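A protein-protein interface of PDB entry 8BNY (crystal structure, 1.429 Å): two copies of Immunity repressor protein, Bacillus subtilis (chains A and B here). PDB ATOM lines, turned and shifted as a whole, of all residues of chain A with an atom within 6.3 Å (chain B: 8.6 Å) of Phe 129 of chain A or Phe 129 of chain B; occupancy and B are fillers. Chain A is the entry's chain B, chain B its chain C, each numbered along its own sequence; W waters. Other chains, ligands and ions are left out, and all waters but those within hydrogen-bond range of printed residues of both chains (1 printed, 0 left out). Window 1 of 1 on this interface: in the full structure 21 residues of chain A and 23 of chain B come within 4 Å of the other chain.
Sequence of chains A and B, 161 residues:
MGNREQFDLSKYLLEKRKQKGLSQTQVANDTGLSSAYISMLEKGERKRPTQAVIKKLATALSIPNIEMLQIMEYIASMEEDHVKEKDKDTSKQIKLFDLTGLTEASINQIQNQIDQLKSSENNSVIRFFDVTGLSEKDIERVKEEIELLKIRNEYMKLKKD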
ATOM      1  N   VAL A 125       7.201 -12.795  37.740  1.00  0.00           N
ATOM      2  CA  VAL A 125       7.499 -12.598  36.325  1.00  0.00           C
ATOM      3  C   VAL A 125       6.651 -13.562  35.508  1.00  0.00           C
ATOM      4  O   VAL A 125       6.619 -14.762  35.796  1.00  0.00           O
ATOM      5  CB  VAL A 125       8.993 -12.831  36.028  1.00  0.00           C
ATOM      6  CG1 VAL A 125       9.210 -13.105  34.549  1.00  0.00           C
ATOM      7  CG2 VAL A 125       9.819 -11.626  36.468  1.00  0.00           C
ATOM      8  N   ILE A 126       5.982 -13.048  34.480  1.00  0.00           N
ATOM      9  CA  ILE A 126       5.277 -13.908  33.541  1.00  0.00           C
ATOM     10  C   ILE A 126       5.899 -13.773  32.156  1.00  0.00           C
ATOM     11  O   ILE A 126       6.487 -12.745  31.801  1.00  0.00           O
ATOM     12  CB  ILE A 126       3.751 -13.660  33.519  1.00  0.00           C
ATOM     13  CG1 ILE A 126       3.415 -12.435  32.678  1.00  0.00           C
ATOM     14  CG2 ILE A 126       3.206 -13.498  34.940  1.00  0.00           C
ATOM     15  CD1 ILE A 126       1.920 -12.192  32.504  1.00  0.00           C
ATOM     16  N   ARG A 127       5.779 -14.838  31.376  1.00  0.00           N
ATOM     17  CA  ARG A 127       6.247 -14.841  30.006  1.00  0.00           C
ATOM     18  C   ARG A 127       5.203 -15.512  29.118  1.00  0.00           C
ATOM     19  O   ARG A 127       4.407 -16.341  29.574  1.00  0.00           O
ATOM     20  CB  ARG A 127       7.622 -15.522  29.846  1.00  0.00           C
ATOM     21  CG  ARG A 127       8.784 -14.609  30.186  1.00  0.00           C
ATOM     22  CD  ARG A 127      10.110 -15.190  29.731  1.00  0.00           C
ATOM     23  NE  ARG A 127      10.196 -15.339  28.282  1.00  0.00           N
ATOM     24  CZ  ARG A 127      11.340 -15.467  27.616  1.00  0.00           C
ATOM     25  NH1 ARG A 127      12.494 -15.450  28.271  1.00  0.00           N
ATOM     26  NH2 ARG A 127      11.332 -15.604  26.295  1.00  0.00           N
ATOM     27  N   PHE A 128       5.203 -15.105  27.857  1.00  0.00           N
ATOM     28  CA  PHE A 128       4.212 -15.552  26.884  1.00  0.00           C
ATOM     29  C   PHE A 128       4.822 -16.590  25.963  1.00  0.00           C
ATOM     30  O   PHE A 128       5.920 -16.381  25.434  1.00  0.00           O
ATOM     31  CB  PHE A 128       3.699 -14.362  26.079  1.00  0.00           C
ATOM     32  CG  PHE A 128       2.853 -13.431  26.884  1.00  0.00           C
ATOM     33  CD1 PHE A 128       3.431 -12.514  27.742  1.00  0.00           C
ATOM     34  CD2 PHE A 128       1.479 -13.487  26.803  1.00  0.00           C
ATOM     35  CE1 PHE A 128       2.658 -11.659  28.491  1.00  0.00           C
ATOM     36  CE2 PHE A 128       0.698 -12.630  27.553  1.00  0.00           C
ATOM     37  CZ  PHE A 128       1.292 -11.715  28.399  1.00  0.00           C
ATOM     38  N   PHE A 129       4.105 -17.704  25.766  1.00  0.00           N
ATOM     39  CA  PHE A 129       4.550 -18.818  24.945  1.00  0.00           C
ATOM     40  C   PHE A 129       3.451 -19.187  23.967  1.00  0.00           C
ATOM     41  O   PHE A 129       2.262 -19.155  24.306  1.00  0.00           O
ATOM     42  CB  PHE A 129       4.848 -20.049  25.792  1.00  0.00           C
ATOM     43  CG  PHE A 129       5.931 -19.844  26.809  1.00  0.00           C
ATOM     44  CD1 PHE A 129       7.258 -19.974  26.456  1.00  0.00           C
ATOM     45  CD2 PHE A 129       5.618 -19.520  28.114  1.00  0.00           C
ATOM     46  CE1 PHE A 129       8.261 -19.791  27.393  1.00  0.00           C
ATOM     47  CE2 PHE A 129       6.614 -19.339  29.063  1.00  0.00           C
ATOM     48  CZ  PHE A 129       7.938 -19.478  28.698  1.00  0.00           C
ATOM     49  N   ASP A 130       3.846 -19.510  22.741  1.00  0.00           N
ATOM     50  CA  ASP A 130       2.911 -20.018  21.756  1.00  0.00           C
ATOM     51  C   ASP A 130       2.631 -21.480  22.086  1.00  0.00           C
ATOM     52  O   ASP A 130       3.551 -22.302  22.129  1.00  0.00           O
ATOM     53  CB  ASP A 130       3.512 -19.878  20.361  1.00  0.00           C
ATOM     54  CG  ASP A 130       2.529 -20.218  19.263  1.00  0.00           C
ATOM     55  OD1 ASP A 130       1.918 -21.309  19.331  1.00  0.00           O
ATOM     56  OD2 ASP A 130       2.357 -19.390  18.338  1.00  0.00           O
ATOM     57  N   VAL A 131       1.369 -21.801  22.348  1.00  0.00           N
ATOM     58  CA  VAL A 131       0.999 -23.163  22.709  1.00  0.00           C
ATOM     59  C   VAL A 131      -0.038 -23.689  21.732  1.00  0.00           C
ATOM     60  O   VAL A 131      -0.911 -24.487  22.104  1.00  0.00           O
ATOM     61  CB  VAL A 131       0.484 -23.241  24.154  1.00  0.00           C
ATOM     62  CG1 VAL A 131       1.633 -23.112  25.121  1.00  0.00           C
ATOM     63  CG2 VAL A 131      -0.582 -22.169  24.382  1.00  0.00           C
ATOM     64  N   THR A 132       0.060 -23.259  20.475  1.00  0.00           N
ATOM     65  CA  THR A 132      -0.945 -23.612  19.487  1.00  0.00           C
ATOM     66  C   THR A 132      -1.069 -25.125  19.397  1.00  0.00           C
ATOM     67  O   THR A 132      -0.067 -25.834  19.272  1.00  0.00           O
ATOM     68  CB  THR A 132      -0.546 -23.039  18.133  1.00  0.00           C
ATOM     69  OG1 THR A 132      -0.374 -21.619  18.257  1.00  0.00           O
ATOM     70  CG2 THR A 132      -1.626 -23.330  17.112  1.00  0.00           C
ATOM     71  N   ILE A 139      -0.940 -28.546  28.322  1.00  0.00           N
ATOM     72  CA  ILE A 139      -0.624 -27.317  29.056  1.00  0.00           C
ATOM     73  C   ILE A 139      -0.260 -27.638  30.498  1.00  0.00           C
ATOM     74  O   ILE A 139       0.681 -27.062  31.061  1.00  0.00           O
ATOM     75  CB  ILE A 139      -1.807 -26.334  28.967  1.00  0.00           C
ATOM     76  CG1 ILE A 139      -2.042 -25.887  27.521  1.00  0.00           C
ATOM     77  CG2 ILE A 139      -1.571 -25.128  29.872  1.00  0.00           C
ATOM     78  CD1 ILE A 139      -0.946 -25.029  26.969  1.00  0.00           C
ATOM     79  N   VAL A 142       3.339 -28.723  30.818  1.00  0.00           N
ATOM     80  CA  VAL A 142       4.235 -27.566  30.794  1.00  0.00           C
ATOM     81  C   VAL A 142       4.285 -26.903  32.164  1.00  0.00           C
ATOM     82  O   VAL A 142       5.361 -26.560  32.666  1.00  0.00           O
ATOM     83  CB  VAL A 142       3.791 -26.563  29.718  1.00  0.00           C
ATOM     84  CG1 VAL A 142       4.655 -25.304  29.793  1.00  0.00           C
ATOM     85  CG2 VAL A 142       3.840 -27.208  28.330  1.00  0.00           C
ATOM     86  N   LYS A 143       3.115 -26.674  32.766  1.00  0.00           N
ATOM     87  CA  LYS A 143       3.070 -26.013  34.069  1.00  0.00           C
ATOM     88  C   LYS A 143       3.816 -26.826  35.112  1.00  0.00           C
ATOM     89  O   LYS A 143       4.528 -26.265  35.955  1.00  0.00           O
ATOM     90  CB  LYS A 143       1.621 -25.773  34.494  1.00  0.00           C
ATOM     91  CG  LYS A 143       0.880 -24.741  33.644  1.00  0.00           C
ATOM     92  CD  LYS A 143      -0.508 -24.458  34.193  1.00  0.00           C
ATOM     93  CE  LYS A 143      -1.330 -23.579  33.253  1.00  0.00           C
ATOM     94  NZ  LYS A 143      -1.155 -22.116  33.524  1.00  0.00           N
ATOM     95  N   ILE A 146       7.578 -26.217  34.645  1.00  0.00           N
ATOM     96  CA  ILE A 146       7.904 -24.946  35.287  1.00  0.00           C
ATOM     97  C   ILE A 146       8.037 -25.126  36.797  1.00  0.00           C
ATOM     98  O   ILE A 146       9.014 -24.684  37.409  1.00  0.00           O
ATOM     99  CB  ILE A 146       6.866 -23.868  34.927  1.00  0.00           C
ATOM    100  CG1 ILE A 146       6.941 -23.546  33.429  1.00  0.00           C
ATOM    101  CG2 ILE A 146       7.077 -22.614  35.795  1.00  0.00           C
ATOM    102  CD1 ILE A 146       5.733 -22.854  32.876  1.00  0.00           C
ATOM    103  N   SER B 124      -2.721 -18.484  15.741  1.00  0.00           N
ATOM    104  CA  SER B 124      -1.858 -18.958  16.816  1.00  0.00           C
ATOM    105  C   SER B 124      -2.476 -18.702  18.184  1.00  0.00           C
ATOM    106  O   SER B 124      -3.203 -17.726  18.369  1.00  0.00           O
ATOM    107  CB  SER B 124      -0.479 -18.294  16.740  1.00  0.00           C
ATOM    108  OG  SER B 124       0.247 -18.757  15.615  1.00  0.00           O
ATOM    109  N   VAL B 125      -2.170 -19.574  19.144  1.00  0.00           N
ATOM    110  CA  VAL B 125      -2.671 -19.454  20.510  1.00  0.00           C
ATOM    111  C   VAL B 125      -1.490 -19.145  21.418  1.00  0.00           C
ATOM    112  O   VAL B 125      -0.501 -19.890  21.442  1.00  0.00           O
ATOM    113  CB  VAL B 125      -3.390 -20.733  20.969  1.00  0.00           C
ATOM    114  CG1 VAL B 125      -3.933 -20.554  22.388  1.00  0.00           C
ATOM    115  CG2 VAL B 125      -4.503 -21.091  19.995  1.00  0.00           C
ATOM    116  N   ILE B 126      -1.589 -18.050  22.161  1.00  0.00           N
ATOM    117  CA  ILE B 126      -0.494 -17.594  23.005  1.00  0.00           C
ATOM    118  C   ILE B 126      -1.005 -17.493  24.431  1.00  0.00           C
ATOM    119  O   ILE B 126      -2.066 -16.900  24.673  1.00  0.00           O
ATOM    120  CB  ILE B 126       0.057 -16.246  22.501  1.00  0.00           C
ATOM    121  CG1 ILE B 126       0.778 -16.475  21.169  1.00  0.00           C
ATOM    122  CG2 ILE B 126       0.992 -15.622  23.524  1.00  0.00           C
ATOM    123  CD1 ILE B 126       1.761 -15.386  20.791  1.00  0.00           C
ATOM    124  N   ARG B 127      -0.260 -18.073  25.373  1.00  0.00           N
ATOM    125  CA  ARG B 127      -0.677 -18.102  26.768  1.00  0.00           C
ATOM    126  C   ARG B 127       0.472 -17.627  27.645  1.00  0.00           C
ATOM    127  O   ARG B 127       1.646 -17.826  27.316  1.00  0.00           O
ATOM    128  CB  ARG B 127      -1.105 -19.520  27.230  1.00  0.00           C
ATOM    129  CG  ARG B 127      -2.422 -20.071  26.662  1.00  0.00           C
ATOM    130  CD  ARG B 127      -3.664 -19.372  27.200  1.00  0.00           C
ATOM    131  NE  ARG B 127      -4.047 -18.261  26.339  1.00  0.00           N
ATOM    132  CZ  ARG B 127      -5.077 -18.261  25.494  1.00  0.00           C
ATOM    133  NH1 ARG B 127      -5.883 -19.313  25.396  1.00  0.00           N
ATOM    134  NH2 ARG B 127      -5.308 -17.185  24.752  1.00  0.00           N
ATOM    135  N   PHE B 128       0.130 -17.020  28.775  1.00  0.00           N
ATOM    136  CA  PHE B 128       1.135 -16.619  29.742  1.00  0.00           C
ATOM    137  C   PHE B 128       1.302 -17.682  30.815  1.00  0.00           C
ATOM    138  O   PHE B 128       0.343 -18.350  31.217  1.00  0.00           O
ATOM    139  CB  PHE B 128       0.837 -15.253  30.374  1.00  0.00           C
ATOM    140  CG  PHE B 128      -0.169 -15.267  31.507  1.00  0.00           C
ATOM    141  CD1 PHE B 128       0.238 -15.481  32.824  1.00  0.00           C
ATOM    142  CD2 PHE B 128      -1.502 -14.978  31.263  1.00  0.00           C
ATOM    143  CE1 PHE B 128      -0.684 -15.455  33.868  1.00  0.00           C
ATOM    144  CE2 PHE B 128      -2.431 -14.950  32.290  1.00  0.00           C
ATOM    145  CZ  PHE B 128      -2.021 -15.198  33.594  1.00  0.00           C
ATOM    146  N   PHE B 129       2.543 -17.806  31.282  1.00  0.00           N
ATOM    147  CA  PHE B 129       2.924 -18.662  32.391  1.00  0.00           C
ATOM    148  C   PHE B 129       3.758 -17.846  33.369  1.00  0.00           C
ATOM    149  O   PHE B 129       4.631 -17.065  32.964  1.00  0.00           O
ATOM    150  CB  PHE B 129       3.765 -19.829  31.890  1.00  0.00           C
ATOM    151  CG  PHE B 129       3.033 -20.748  30.956  1.00  0.00           C
ATOM    152  CD1 PHE B 129       2.862 -20.403  29.621  1.00  0.00           C
ATOM    153  CD2 PHE B 129       2.513 -21.950  31.411  1.00  0.00           C
ATOM    154  CE1 PHE B 129       2.188 -21.229  28.750  1.00  0.00           C
ATOM    155  CE2 PHE B 129       1.839 -22.793  30.547  1.00  0.00           C
ATOM    156  CZ  PHE B 129       1.675 -22.435  29.209  1.00  0.00           C
ATOM    157  N   ASP B 130       3.477 -18.011  34.653  1.00  0.00           N
ATOM    158  CA  ASP B 130       4.354 -17.464  35.678  1.00  0.00           C
ATOM    159  C   ASP B 130       5.657 -18.252  35.680  1.00  0.00           C
ATOM    160  O   ASP B 130       5.656 -19.477  35.868  1.00  0.00           O
ATOM    161  CB  ASP B 130       3.676 -17.533  37.042  1.00  0.00           C
ATOM    162  CG  ASP B 130       4.429 -16.768  38.104  1.00  0.00           C
ATOM    163  OD1 ASP B 130       5.666 -16.951  38.236  1.00  0.00           O
ATOM    164  OD2 ASP B 130       3.784 -15.968  38.820  1.00  0.00           O
ATOM    165  N   VAL B 131       6.767 -17.550  35.461  1.00  0.00           N
ATOM    166  CA  VAL B 131       8.075 -18.187  35.401  1.00  0.00           C
ATOM    167  C   VAL B 131       9.014 -17.552  36.415  1.00  0.00           C
ATOM    168  O   VAL B 131      10.221 -17.434  36.162  1.00  0.00           O
ATOM    169  CB  VAL B 131       8.677 -18.098  33.987  1.00  0.00           C
ATOM    170  CG1 VAL B 131       7.956 -19.053  33.042  1.00  0.00           C
ATOM    171  CG2 VAL B 131       8.629 -16.662  33.490  1.00  0.00           C
ATOM    172  N   THR B 132       8.480 -17.145  37.563  1.00  0.00           N
ATOM    173  CA  THR B 132       9.290 -16.401  38.520  1.00  0.00           C
ATOM    174  C   THR B 132      10.508 -17.211  38.953  1.00  0.00           C
ATOM    175  O   THR B 132      10.418 -18.407  39.248  1.00  0.00           O
ATOM    176  CB  THR B 132       8.458 -16.001  39.736  1.00  0.00           C
ATOM    177  OG1 THR B 132       7.305 -15.266  39.307  1.00  0.00           O
ATOM    178  CG2 THR B 132       9.293 -15.119  40.671  1.00  0.00           C
ATOM    179  N   LEU B 134      12.934 -18.308  37.190  1.00  0.00           N
ATOM    180  CA  LEU B 134      13.509 -19.170  36.167  1.00  0.00           C
ATOM    181  C   LEU B 134      14.591 -18.420  35.399  1.00  0.00           C
ATOM    182  O   LEU B 134      14.384 -17.275  34.980  1.00  0.00           O
ATOM    183  CB  LEU B 134      12.435 -19.654  35.190  1.00  0.00           C
ATOM    184  CG  LEU B 134      11.885 -21.047  35.460  1.00  0.00           C
ATOM    185  CD1 LEU B 134      11.184 -21.073  36.791  1.00  0.00           C
ATOM    186  CD2 LEU B 134      10.951 -21.508  34.331  1.00  0.00           C
ATOM    187  N   SER B 135      15.734 -19.076  35.204  1.00  0.00           N
ATOM    188  CA  SER B 135      16.787 -18.536  34.363  1.00  0.00           C
ATOM    189  C   SER B 135      16.390 -18.678  32.899  1.00  0.00           C
ATOM    190  O   SER B 135      15.479 -19.439  32.546  1.00  0.00           O
ATOM    191  CB  SER B 135      18.084 -19.313  34.581  1.00  0.00           C
ATOM    192  OG  SER B 135      18.053 -20.535  33.882  1.00  0.00           O
ATOM    193  N   GLU B 136      17.100 -17.947  32.033  1.00  0.00           N
ATOM    194  CA  GLU B 136      16.892 -18.103  30.595  1.00  0.00           C
ATOM    195  C   GLU B 136      17.052 -19.549  30.152  1.00  0.00           C
ATOM    196  O   GLU B 136      16.308 -20.015  29.281  1.00  0.00           O
ATOM    197  CB  GLU B 136      17.818 -17.190  29.797  1.00  0.00           C
ATOM    198  CG  GLU B 136      17.299 -15.760  29.682  1.00  0.00           C
ATOM    199  CD  GLU B 136      15.800 -15.706  29.399  1.00  0.00           C
ATOM    200  OE1 GLU B 136      15.362 -16.224  28.344  1.00  0.00           O
ATOM    201  OE2 GLU B 136      15.059 -15.160  30.250  1.00  0.00           O
ATOM    202  N   ASP B 138      16.409 -22.272  32.019  1.00  0.00           N
ATOM    203  CA  ASP B 138      15.172 -22.956  32.392  1.00  0.00           C
ATOM    204  C   ASP B 138      14.045 -22.629  31.412  1.00  0.00           C
ATOM    205  O   ASP B 138      13.268 -23.521  31.033  1.00  0.00           O
ATOM    206  CB  ASP B 138      14.734 -22.559  33.801  1.00  0.00           C
ATOM    207  CG  ASP B 138      15.794 -22.840  34.867  1.00  0.00           C
ATOM    208  OD1 ASP B 138      16.579 -23.806  34.722  1.00  0.00           O
ATOM    209  OD2 ASP B 138      15.841 -22.079  35.861  1.00  0.00           O
ATOM    210  N   ILE B 139      13.938 -21.361  31.004  1.00  0.00           N
ATOM    211  CA  ILE B 139      12.943 -20.971  30.007  1.00  0.00           C
ATOM    212  C   ILE B 139      13.128 -21.789  28.738  1.00  0.00           C
ATOM    213  O   ILE B 139      12.168 -22.358  28.205  1.00  0.00           O
ATOM    214  CB  ILE B 139      13.004 -19.458  29.722  1.00  0.00           C
ATOM    215  CG1 ILE B 139      12.645 -18.642  30.972  1.00  0.00           C
ATOM    216  CG2 ILE B 139      12.069 -19.099  28.559  1.00  0.00           C
ATOM    217  CD1 ILE B 139      11.215 -18.826  31.432  1.00  0.00           C
ATOM    218  N   GLU B 140      14.373 -21.868  28.242  1.00  0.00           N
ATOM    219  CA  GLU B 140      14.659 -22.675  27.054  1.00  0.00           C
ATOM    220  C   GLU B 140      14.166 -24.106  27.212  1.00  0.00           C
ATOM    221  O   GLU B 140      13.640 -24.699  26.263  1.00  0.00           O
ATOM    222  CB  GLU B 140      16.152 -22.678  26.741  1.00  0.00           C
ATOM    223  CG  GLU B 140      16.748 -21.304  26.442  1.00  0.00           C
ATOM    224  CD  GLU B 140      15.870 -20.435  25.536  1.00  0.00           C
ATOM    225  OE1 GLU B 140      15.377 -20.941  24.497  1.00  0.00           O
ATOM    226  OE2 GLU B 140      15.676 -19.238  25.869  1.00  0.00           O
ATOM    227  N   ARG B 141      14.321 -24.685  28.407  1.00  0.00           N
ATOM    228  CA  ARG B 141      13.827 -26.041  28.632  1.00  0.00           C
ATOM    229  C   ARG B 141      12.301 -26.120  28.510  1.00  0.00           C
ATOM    230  O   ARG B 141      11.759 -27.095  27.970  1.00  0.00           O
ATOM    231  CB  ARG B 141      14.269 -26.526  30.008  1.00  0.00           C
ATOM    232  CG  ARG B 141      13.952 -27.984  30.241  1.00  0.00           C
ATOM    233  CD  ARG B 141      14.422 -28.465  31.596  1.00  0.00           C
ATOM    234  NE  ARG B 141      14.097 -29.883  31.745  1.00  0.00           N
ATOM    235  CZ  ARG B 141      14.908 -30.869  31.376  1.00  0.00           C
ATOM    236  NH1 ARG B 141      16.096 -30.582  30.858  1.00  0.00           N
ATOM    237  NH2 ARG B 141      14.536 -32.135  31.529  1.00  0.00           N
ATOM    238  N   VAL B 142      11.598 -25.103  29.017  1.00  0.00           N
ATOM    239  CA  VAL B 142      10.145 -25.025  28.875  1.00  0.00           C
ATOM    240  C   VAL B 142       9.739 -24.940  27.399  1.00  0.00           C
ATOM    241  O   VAL B 142       8.874 -25.703  26.934  1.00  0.00           O
ATOM    242  CB  VAL B 142       9.608 -23.848  29.704  1.00  0.00           C
ATOM    243  CG1 VAL B 142       8.127 -23.729  29.548  1.00  0.00           C
ATOM    244  CG2 VAL B 142       9.970 -24.049  31.179  1.00  0.00           C
ATOM    245  N   LYS B 143      10.362 -24.024  26.636  1.00  0.00           N
ATOM    246  CA  LYS B 143      10.102 -23.932  25.198  1.00  0.00           C
ATOM    247  C   LYS B 143      10.315 -25.271  24.493  1.00  0.00           C
ATOM    248  O   LYS B 143       9.496 -25.679  23.655  1.00  0.00           O
ATOM    249  CB  LYS B 143      10.942 -22.828  24.548  1.00  0.00           C
ATOM    250  CG  LYS B 143      10.609 -21.408  24.994  1.00  0.00           C
ATOM    251  CD  LYS B 143      11.395 -20.388  24.173  1.00  0.00           C
ATOM    252  CE  LYS B 143      11.384 -19.005  24.784  1.00  0.00           C
ATOM    253  NZ  LYS B 143      12.310 -18.102  24.049  1.00  0.00           N
ATOM    254  N   GLU B 144      11.391 -25.991  24.843  1.00  0.00           N
ATOM    255  CA  GLU B 144      11.660 -27.287  24.232  1.00  0.00           C
ATOM    256  C   GLU B 144      10.566 -28.294  24.570  1.00  0.00           C
ATOM    257  O   GLU B 144      10.197 -29.126  23.734  1.00  0.00           O
ATOM    258  CB  GLU B 144      13.023 -27.820  24.691  1.00  0.00           C
ATOM    259  CG  GLU B 144      13.464 -29.067  23.947  1.00  0.00           C
ATOM    260  CD  GLU B 144      13.907 -28.768  22.519  1.00  0.00           C
ATOM    261  OE1 GLU B 144      14.334 -27.620  22.254  1.00  0.00           O
ATOM    262  OE2 GLU B 144      13.823 -29.678  21.664  1.00  0.00           O
ATOM    263  N   ILE B 146       7.395 -27.570  25.198  1.00  0.00           N
ATOM    264  CA  ILE B 146       6.276 -27.178  24.343  1.00  0.00           C
ATOM    265  C   ILE B 146       6.473 -27.688  22.919  1.00  0.00           C
ATOM    266  O   ILE B 146       5.546 -28.242  22.315  1.00  0.00           O
ATOM    267  CB  ILE B 146       6.059 -25.655  24.393  1.00  0.00           C
ATOM    268  CG1 ILE B 146       5.628 -25.206  25.815  1.00  0.00           C
ATOM    269  CG2 ILE B 146       5.049 -25.234  23.301  1.00  0.00           C
ATOM    270  CD1 ILE B 146       5.682 -23.696  26.071  1.00  0.00           C
ATOM    271  N   LYS B 150       3.982 -30.172  20.829  1.00  0.00           N
ATOM    272  CA  LYS B 150       3.450 -29.876  19.499  1.00  0.00           C
ATOM    273  C   LYS B 150       3.784 -30.977  18.493  1.00  0.00           C
ATOM    274  O   LYS B 150       2.938 -31.338  17.663  1.00  0.00           O
ATOM    275  CB  LYS B 150       3.950 -28.530  18.988  1.00  0.00           C
ATOM    276  CG  LYS B 150       3.422 -27.317  19.760  1.00  0.00           C
ATOM    277  CD  LYS B 150       3.981 -26.014  19.202  1.00  0.00           C
ATOM    278  CE  LYS B 150       3.352 -24.782  19.815  1.00  0.00           C
ATOM    279  NZ  LYS B 150       3.795 -23.585  19.073  1.00  0.00           N
HETATM  280  O   HOH W   1       0.904 -19.958  35.114  1.00  0.00           O
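The backbone carbonyl oxygen of Val 125 of chain A is in hydrogen-bond range of the backbone NH of Val 131 of chain B (2.8 Å). N of Val 125 of chain A sits at hydrogen-bond distance from OG1 of Thr 132 of chain B, 2.9 Å away. The backbone NH of Phe 129 of chain B sits at hydrogen-bond distance from the backbone carbonyl oxygen of Arg 127 of chain A, 2.9 Å away. The side-chain carboxylate (OE1) of Glu 136 of chain B lies within salt-bridge range of the guanidinium group (NH1) of Arg 127 of chain A, 3.0 Å away. N of Phe 129 of chain A is in hydrogen-bond range of O of Arg 127 of chain B (2.9 Å). The side-chain carboxylate (OD1) of Asp 130 of chain A is in salt-bridge range of the side-chain amino group (NZ) of Lys 150 of chain B. N of Val 131 of chain A lies within hydrogen-bond range of O of Val 125 of chain B (2.8 Å). OG1 of Thr 132 of chain A sits at hydrogen-bond distance from N of Val 125 of chain B, 2.9 Å away. The side-chain carboxylate (OD1) of Asp 130 of chain B sits close to the backbone carbonyl oxygen (O) of Val 125 of chain A (3.4 Å). The guanidinium group (NH2) of Arg 127 of chain A sits close to the side-chain amino group (NZ) of Lys 143 of chain B, at 3.5 Å.
Arg 127 of chain A touches Phe 128 of chain B, and with the chains exchanged Phe 128 of chain A touches Arg 127 of chain B. Arg 127 of chain A touches Phe 129 of chain B, and with the chains exchanged Phe 129 of chain A touches Arg 127 of chain B. Arg 127 of chain A touches Val 131 of chain B, and with the chains exchanged Val 131 of chain A touches Arg 127 of chain B. Of the 36 pairs that touch across the chains among the printed residues, 28 have their exchanged pair printed and touching as well.
Of the 12 printed residues of chain A, 11 touch a printed residue of chain B. Of the 21 printed residues of chain B, 15 touch a printed residue of chain A. Printed residues of chain B that touch a printed residue of chain A: Ser 124, Val 125, Ile 126, Arg 127, Phe 128, Phe 129, Asp 130, Val 131, Thr 132, Glu 136, Ile 139, Val 142, Lys 143, Ile 146 and Lys 150. Among the printed residues, Asp or Glu carboxylates within 4 Å of a Lys or Arg side-chain nitrogen of the other chain: Arg 127 of chain A with Glu 136 of chain B and Asp 130 of chain A with Lys 150 of chain B.
Of the printed residues of chain B, Arg 127 of chain A touches Arg 127, Phe 128, Phe 129, Val 131, Glu 136, Ile 139 and Lys 143. Phe 129 of chain A touches just these residues of chain B: Ile 126 (3.4 Å), Arg 127 (2.9 Å), Phe 129 (3.3 Å), Lys 143 (3.7 Å) and Ile 146 (3.8 Å). Printed residues of chain B within 4 Å of Asp 130 of chain A: Ser 124 (3.4 Å), Val 125 (3.4 Å), Ile 146 (3.5 Å) and Lys 150 (3.0 Å). Printed residues of chain A within 4 Å of Phe 129 of chain B: Ile 126, Arg 127, Phe 129, Val 142, Lys 143 and Ile 146. Printed residues of chain A within 4 Å of Thr 132 of chain B: Val 125 (2.9 Å). The nearest printed residue of chain A that does not touch Phe 129 of chain B is Val 131 of chain A (4.1 Å). The nearest printed residue of chain A that does not touch Ile 139 of chain B is Phe 129 of chain A (4.04 Å).
OD1 of Asp 130 of chain A sits at hydrogen-bond distance from OG1 of Thr 132 of chain A. OG1 of Thr 132 of chain B lies within hydrogen-bond range of OD1 of Asp 130 of chain B (2.6 Å). The side-chain amino group of Lys 143 of chain B lies within salt-bridge range of the side-chain carboxylate of Glu 140 of chain B.
Among the printed residues, merely in contact across the chains: Ile 126 of chain A with Phe 128 of chain B, Ile 126 of chain A with Phe 129 of chain B, Arg 127 of chain A with Arg 127 of chain B, Arg 127 of chain A with Phe 128 of chain B, Arg 127 of chain A with Val 131 of chain B, Arg 127 of chain A with Ile 139 of chain B, Phe 128 of chain A with Ile 126 of chain B, Phe 128 of chain A with Arg 127 of chain B, Phe 128 of chain A with Phe 128 of chain B, Phe 129 of chain A with Ile 126 of chain B, Phe 129 of chain A with Phe 129 of chain B, Phe 129 of chain A with Lys 143 of chain B, Phe 129 of chain A with Ile 146 of chain B, Asp 130 of chain A with Ser 124 of chain B, Asp 130 of chain A with Val 125 of chain B, Asp 130 of chain A with Ile 146 of chain B, Val 131 of chain A with Arg 127 of chain B, Thr 132 of chain A with Ser 124 of chain B, Thr 132 of chain A with Lys 150 of chain B, Val 142 of chain A with Phe 129 of chain B, Val 142 of chain A with Val 142 of chain B, Val 142 of chain A with Ile 146 of chain B, Lys 143 of chain A with Phe 129 of chain B, Ile 146 of chain A with Phe 129 of chain B, Ile 146 of chain A with Asp 130 of chain B and Ile 146 of chain A with Val 142 of chain B.
Water W1 lies within hydrogen-bond range of the backbone NH (N) of Asp 130 of chain B (3.3 Å) and the side-chain amino group (NZ) of Lys 143 of chain A (3.4 Å).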
